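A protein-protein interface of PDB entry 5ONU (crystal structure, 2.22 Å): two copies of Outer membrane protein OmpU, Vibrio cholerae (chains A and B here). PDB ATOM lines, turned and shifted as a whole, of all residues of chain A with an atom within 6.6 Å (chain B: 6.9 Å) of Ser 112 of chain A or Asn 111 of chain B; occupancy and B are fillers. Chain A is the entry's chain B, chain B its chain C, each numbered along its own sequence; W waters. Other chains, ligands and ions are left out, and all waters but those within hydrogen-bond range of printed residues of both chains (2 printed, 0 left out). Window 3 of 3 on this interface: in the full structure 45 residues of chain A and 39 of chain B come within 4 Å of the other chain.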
ATOM      1  N   GLU A  98      -8.103   3.489  18.480  1.00  0.00           N
ATOM      2  CA  GLU A  98      -8.146   3.695  19.928  1.00  0.00           C
ATOM      3  C   GLU A  98      -7.223   4.841  20.357  1.00  0.00           C
ATOM      4  O   GLU A  98      -6.096   4.963  19.864  1.00  0.00           O
ATOM      5  CB  GLU A  98      -7.771   2.405  20.665  1.00  0.00           C
ATOM      6  CG  GLU A  98      -7.844   2.509  22.181  1.00  0.00           C
ATOM      7  CD  GLU A  98      -7.698   1.163  22.867  1.00  0.00           C
ATOM      8  OE1 GLU A  98      -6.648   0.929  23.501  1.00  0.00           O
ATOM      9  OE2 GLU A  98      -8.637   0.344  22.779  1.00  0.00           O
ATOM     10  N   PHE A  99      -7.715   5.671  21.278  1.00  0.00           N
ATOM     11  CA  PHE A  99      -7.044   6.909  21.678  1.00  0.00           C
ATOM     12  C   PHE A  99      -6.873   6.987  23.200  1.00  0.00           C
ATOM     13  O   PHE A  99      -7.828   6.753  23.943  1.00  0.00           O
ATOM     14  CB  PHE A  99      -7.836   8.128  21.189  1.00  0.00           C
ATOM     15  CG  PHE A  99      -8.188   8.091  19.724  1.00  0.00           C
ATOM     16  CD1 PHE A  99      -9.252   7.322  19.268  1.00  0.00           C
ATOM     17  CD2 PHE A  99      -7.466   8.833  18.803  1.00  0.00           C
ATOM     18  CE1 PHE A  99      -9.580   7.288  17.925  1.00  0.00           C
ATOM     19  CE2 PHE A  99      -7.791   8.803  17.458  1.00  0.00           C
ATOM     20  CZ  PHE A  99      -8.849   8.029  17.019  1.00  0.00           C
ATOM     21  N   THR A 100      -5.671   7.325  23.665  1.00  0.00           N
ATOM     22  CA  THR A 100      -5.389   7.390  25.106  1.00  0.00           C
ATOM     23  C   THR A 100      -4.552   8.603  25.522  1.00  0.00           C
ATOM     24  O   THR A 100      -3.970   9.289  24.681  1.00  0.00           O
ATOM     25  CB  THR A 100      -4.650   6.125  25.596  1.00  0.00           C
ATOM     26  OG1 THR A 100      -3.419   5.982  24.876  1.00  0.00           O
ATOM     27  CG2 THR A 100      -5.500   4.876  25.398  1.00  0.00           C
ATOM     28  N   THR A 101      -4.504   8.859  26.829  1.00  0.00           N
ATOM     29  CA  THR A 101      -3.641   9.900  27.390  1.00  0.00           C
ATOM     30  C   THR A 101      -2.664   9.341  28.428  1.00  0.00           C
ATOM     31  O   THR A 101      -2.891   8.272  28.995  1.00  0.00           O
ATOM     32  CB  THR A 101      -4.460  11.025  28.060  1.00  0.00           C
ATOM     33  OG1 THR A 101      -5.063  10.531  29.263  1.00  0.00           O
ATOM     34  CG2 THR A 101      -5.539  11.541  27.122  1.00  0.00           C
ATOM     35  N   ASN A 102      -1.583  10.079  28.670  1.00  0.00           N
ATOM     36  CA  ASN A 102      -0.607   9.727  29.697  1.00  0.00           C
ATOM     37  C   ASN A 102       0.093  10.981  30.228  1.00  0.00           C
ATOM     38  O   ASN A 102       1.270  11.213  29.948  1.00  0.00           O
ATOM     39  CB  ASN A 102       0.418   8.731  29.144  1.00  0.00           C
ATOM     40  CG  ASN A 102       1.358   8.200  30.212  1.00  0.00           C
ATOM     41  OD1 ASN A 102       0.952   7.955  31.349  1.00  0.00           O
ATOM     42  ND2 ASN A 102       2.622   8.017  29.849  1.00  0.00           N
ATOM     43  N   ASN A 110      -0.686  14.628  23.886  1.00  0.00           N
ATOM     44  CA  ASN A 110      -0.800  13.173  23.859  1.00  0.00           C
ATOM     45  C   ASN A 110      -1.041  12.631  22.453  1.00  0.00           C
ATOM     46  O   ASN A 110      -2.147  12.719  21.919  1.00  0.00           O
ATOM     47  CB  ASN A 110      -1.915  12.715  24.802  1.00  0.00           C
ATOM     48  CG  ASN A 110      -1.516  12.811  26.264  1.00  0.00           C
ATOM     49  OD1 ASN A 110      -0.741  11.994  26.762  1.00  0.00           O
ATOM     50  ND2 ASN A 110      -2.041  13.814  26.959  1.00  0.00           N
ATOM     51  N   ASN A 111       0.011  12.071  21.864  1.00  0.00           N
ATOM     52  CA  ASN A 111      -0.020  11.593  20.486  1.00  0.00           C
ATOM     53  C   ASN A 111      -0.174  10.071  20.418  1.00  0.00           C
ATOM     54  O   ASN A 111       0.558   9.397  19.693  1.00  0.00           O
ATOM     55  CB  ASN A 111       1.255  12.031  19.758  1.00  0.00           C
ATOM     56  CG  ASN A 111       1.106  12.025  18.244  1.00  0.00           C
ATOM     57  OD1 ASN A 111       0.289  11.293  17.686  1.00  0.00           O
ATOM     58  ND2 ASN A 111       1.907  12.844  17.572  1.00  0.00           N
ATOM     59  N   SER A 112      -1.118   9.532  21.184  1.00  0.00           N
ATOM     60  CA  SER A 112      -1.292   8.084  21.285  1.00  0.00           C
ATOM     61  C   SER A 112      -2.470   7.563  20.457  1.00  0.00           C
ATOM     62  O   SER A 112      -3.629   7.838  20.768  1.00  0.00           O
ATOM     63  CB  SER A 112      -1.470   7.679  22.750  1.00  0.00           C
ATOM     64  OG  SER A 112      -1.936   6.345  22.859  1.00  0.00           O
ATOM     65  N   LEU A 113      -2.162   6.809  19.405  1.00  0.00           N
ATOM     66  CA  LEU A 113      -3.180   6.254  18.514  1.00  0.00           C
ATOM     67  C   LEU A 113      -2.897   4.787  18.185  1.00  0.00           C
ATOM     68  O   LEU A 113      -1.746   4.406  17.977  1.00  0.00           O
ATOM     69  CB  LEU A 113      -3.260   7.077  17.223  1.00  0.00           C
ATOM     70  CG  LEU A 113      -3.964   6.445  16.019  1.00  0.00           C
ATOM     71  CD1 LEU A 113      -5.470   6.405  16.224  1.00  0.00           C
ATOM     72  CD2 LEU A 113      -3.613   7.188  14.737  1.00  0.00           C
ATOM     73  N   ASP A 114      -3.943   3.963  18.145  1.00  0.00           N
ATOM     74  CA  ASP A 114      -3.792   2.577  17.696  1.00  0.00           C
ATOM     75  C   ASP A 114      -4.852   2.189  16.663  1.00  0.00           C
ATOM     76  O   ASP A 114      -6.041   2.134  16.972  1.00  0.00           O
ATOM     77  CB  ASP A 114      -3.847   1.618  18.888  1.00  0.00           C
ATOM     78  CG  ASP A 114      -3.596   0.170  18.489  1.00  0.00           C
ATOM     79  OD1 ASP A 114      -3.027  -0.064  17.402  1.00  0.00           O
ATOM     80  OD2 ASP A 114      -3.967  -0.735  19.266  1.00  0.00           O
ATOM     81  N   ASN A 115      -4.410   1.919  15.437  1.00  0.00           N
ATOM     82  CA  ASN A 115      -5.296   1.451  14.371  1.00  0.00           C
ATOM     83  C   ASN A 115      -5.597  -0.044  14.499  1.00  0.00           C
ATOM     84  O   ASN A 115      -4.862  -0.877  13.971  1.00  0.00           O
ATOM     85  CB  ASN A 115      -4.676   1.740  13.002  1.00  0.00           C
ATOM     86  CG  ASN A 115      -4.369   3.214  12.795  1.00  0.00           C
ATOM     87  OD1 ASN A 115      -5.151   4.085  13.176  1.00  0.00           O
ATOM     88  ND2 ASN A 115      -3.220   3.498  12.192  1.00  0.00           N
ATOM     89  N   THR B 100      -2.780   3.629   8.592  1.00  0.00           N
ATOM     90  CA  THR B 100      -2.205   2.363   8.122  1.00  0.00           C
ATOM     91  C   THR B 100      -1.699   1.469   9.259  1.00  0.00           C
ATOM     92  O   THR B 100      -1.555   1.917  10.397  1.00  0.00           O
ATOM     93  CB  THR B 100      -1.027   2.597   7.149  1.00  0.00           C
ATOM     94  OG1 THR B 100      -0.003   3.353   7.807  1.00  0.00           O
ATOM     95  CG2 THR B 100      -1.484   3.342   5.900  1.00  0.00           C
ATOM     96  N   SER B 109       0.803  -2.592  18.196  1.00  0.00           N
ATOM     97  CA  SER B 109       0.152  -1.293  18.252  1.00  0.00           C
ATOM     98  C   SER B 109       0.620  -0.462  17.063  1.00  0.00           C
ATOM     99  O   SER B 109       1.813  -0.417  16.766  1.00  0.00           O
ATOM    100  CB  SER B 109       0.465  -0.584  19.570  1.00  0.00           C
ATOM    101  OG  SER B 109      -0.537   0.362  19.894  1.00  0.00           O
ATOM    102  N   ASN B 110      -0.314   0.194  16.384  1.00  0.00           N
ATOM    103  CA  ASN B 110       0.016   0.922  15.164  1.00  0.00           C
ATOM    104  C   ASN B 110      -0.362   2.398  15.246  1.00  0.00           C
ATOM    105  O   ASN B 110      -1.534   2.763  15.137  1.00  0.00           O
ATOM    106  CB  ASN B 110      -0.664   0.267  13.960  1.00  0.00           C
ATOM    107  CG  ASN B 110       0.002  -1.037  13.554  1.00  0.00           C
ATOM    108  OD1 ASN B 110       1.080  -1.038  12.961  1.00  0.00           O
ATOM    109  ND2 ASN B 110      -0.639  -2.155  13.879  1.00  0.00           N
ATOM    110  N   ASN B 111       0.649   3.240  15.439  1.00  0.00           N
ATOM    111  CA  ASN B 111       0.451   4.671  15.642  1.00  0.00           C
ATOM    112  C   ASN B 111       0.748   5.463  14.368  1.00  0.00           C
ATOM    113  O   ASN B 111       1.460   6.467  14.404  1.00  0.00           O
ATOM    114  CB  ASN B 111       1.339   5.157  16.792  1.00  0.00           C
ATOM    115  CG  ASN B 111       0.860   6.466  17.399  1.00  0.00           C
ATOM    116  OD1 ASN B 111       0.194   7.268  16.744  1.00  0.00           O
ATOM    117  ND2 ASN B 111       1.205   6.688  18.663  1.00  0.00           N
ATOM    118  N   SER B 112       0.212   5.001  13.242  1.00  0.00           N
ATOM    119  CA  SER B 112       0.501   5.615  11.948  1.00  0.00           C
ATOM    120  C   SER B 112      -0.633   6.507  11.439  1.00  0.00           C
ATOM    121  O   SER B 112      -1.706   6.021  11.078  1.00  0.00           O
ATOM    122  CB  SER B 112       0.809   4.534  10.910  1.00  0.00           C
ATOM    123  OG  SER B 112       0.800   5.073   9.598  1.00  0.00           O
ATOM    124  N   LEU B 113      -0.379   7.811  11.405  1.00  0.00           N
ATOM    125  CA  LEU B 113      -1.365   8.791  10.954  1.00  0.00           C
ATOM    126  C   LEU B 113      -0.733   9.815  10.015  1.00  0.00           C
ATOM    127  O   LEU B 113       0.394  10.254  10.241  1.00  0.00           O
ATOM    128  CB  LEU B 113      -1.999   9.501  12.153  1.00  0.00           C
ATOM    129  CG  LEU B 113      -2.736  10.814  11.869  1.00  0.00           C
ATOM    130  CD1 LEU B 113      -4.059  10.557  11.165  1.00  0.00           C
ATOM    131  CD2 LEU B 113      -2.949  11.607  13.150  1.00  0.00           C
HETATM  132  O   HOH W   1      -3.221  -2.393  15.533  1.00  0.00           O
HETATM  133  O   HOH W   2       0.319   3.157  19.624  1.00  0.00           O
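Among the printed residues, merely in contact across the chains: Asp 114 of chain A with Ser 109 of chain B, Leu 113 of chain A with Leu 113 of chain B and Ser 112 of chain A with Asn 111 of chain B.
Water W1 lies within hydrogen-bond range of O of Asn 115 of chain A (2.7 Å), OD1 of Asp 114 of chain A (3.0 Å) and ND2 of Asn 110 of chain B (3.1 Å). Water W2 lies within hydrogen-bond range of the backbone carbonyl oxygen (O) of Leu 113 of chain A (2.9 Å) and the side-chain hydroxyl (OG) of Ser 109 of chain B (2.9 Å).
Ser 112 of chain A touches just one residue of chain B: Asn 111 (3.9 Å). Printed residues of chain B within 4 Å of Asp 114 of chain A: Ser 109 and Asn 110. Of the printed residues of chain A, Asn 110 of chain B touches Leu 113 (3.3 Å), Asp 114 (2.9 Å) and Asn 115 (3.0 Å). Of the printed residues of chain A, Asn 111 of chain B touches Asn 111 (3.0 Å), Ser 112 (3.9 Å) and Leu 113 (3.2 Å). The nearest residue of chain B that does not touch Ser 112 of chain A is Ser 109 of chain B (6.8 Å).
Asn 111 of chain A touches its own counterpart, Asn 111 of chain B. Ser 112 of chain A touches Asn 111 of chain B, but with the chains exchanged Asn 111 of chain A does not touch Ser 112 of chain B (7.7 Å). Leu 113 of chain A touches Asn 110 of chain B, but with the chains exchanged Asn 110 of chain A does not touch Leu 113 of chain B (8.9 Å). Leu 113 of chain A touches Asn 111 of chain B, but with the chains exchanged Asn 111 of chain A does not touch Leu 113 of chain B (5.6 Å). Of the 10 pairs that touch across the chains among the printed residues, 2 have their exchanged pair printed and touching as well.
Of the 6 printed residues of chain B, 6 touch a printed residue of chain A. Printed residues of chain B that touch a printed residue of chain A: Thr 100, Ser 109, Asn 110, Asn 111, Ser 112 and Leu 113. Hydrophobic or aromatic side chains of chain B that line the printed part of chain A: Leu 113. Printed residues of chain A that touch a printed residue of chain B: Asn 111, Ser 112, Leu 113, Asp 114 and Asn 115. Among the printed residues, 10 pairs touch across the chains. Among the printed residues, no Asp or Glu carboxylate lies within 4 Å of a Lys or Arg side-chain nitrogen of the other chain.
The side-chain hydroxyl (OG1) of Thr 100 of chain A is in hydrogen-bond range of the side-chain hydroxyl (OG) of Ser 112 of chain A. OG1 of Thr 100 of chain B sits at hydrogen-bond distance from OG of Ser 112 of chain B, at 2.6 Å. N of Glu 98 of chain A sits at hydrogen-bond distance from O of Asp 114 of chain A, at 2.9 Å.
O of Asn 111 of chain A is in hydrogen-bond range of ND2 of Asn 111 of chain B (3.0 Å). The backbone carbonyl oxygen (O) of Thr 100 of chain B lies within hydrogen-bond range of the side-chain amide nitrogen (ND2) of Asn 115 of chain A, at 2.9 Å. N of Asn 115 of chain A lies within hydrogen-bond range of O of Asn 110 of chain B (3.0 Å). The side-chain carboxylate (OD1) of Asp 114 of chain A is in hydrogen-bond range of the backbone NH (N) of Asn 110 of chain B (2.9 Å). O of Asn 110 of chain B lies close to O of Leu 113 of chain A, at 3.3 Å. N of Leu 113 of chain A lies close to ND2 of Asn 111 of chain B (3.4 Å). ND2 of Asn 115 of chain A lies within hydrogen-bond range of O of Ser 112 of chain B (3.1 Å).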
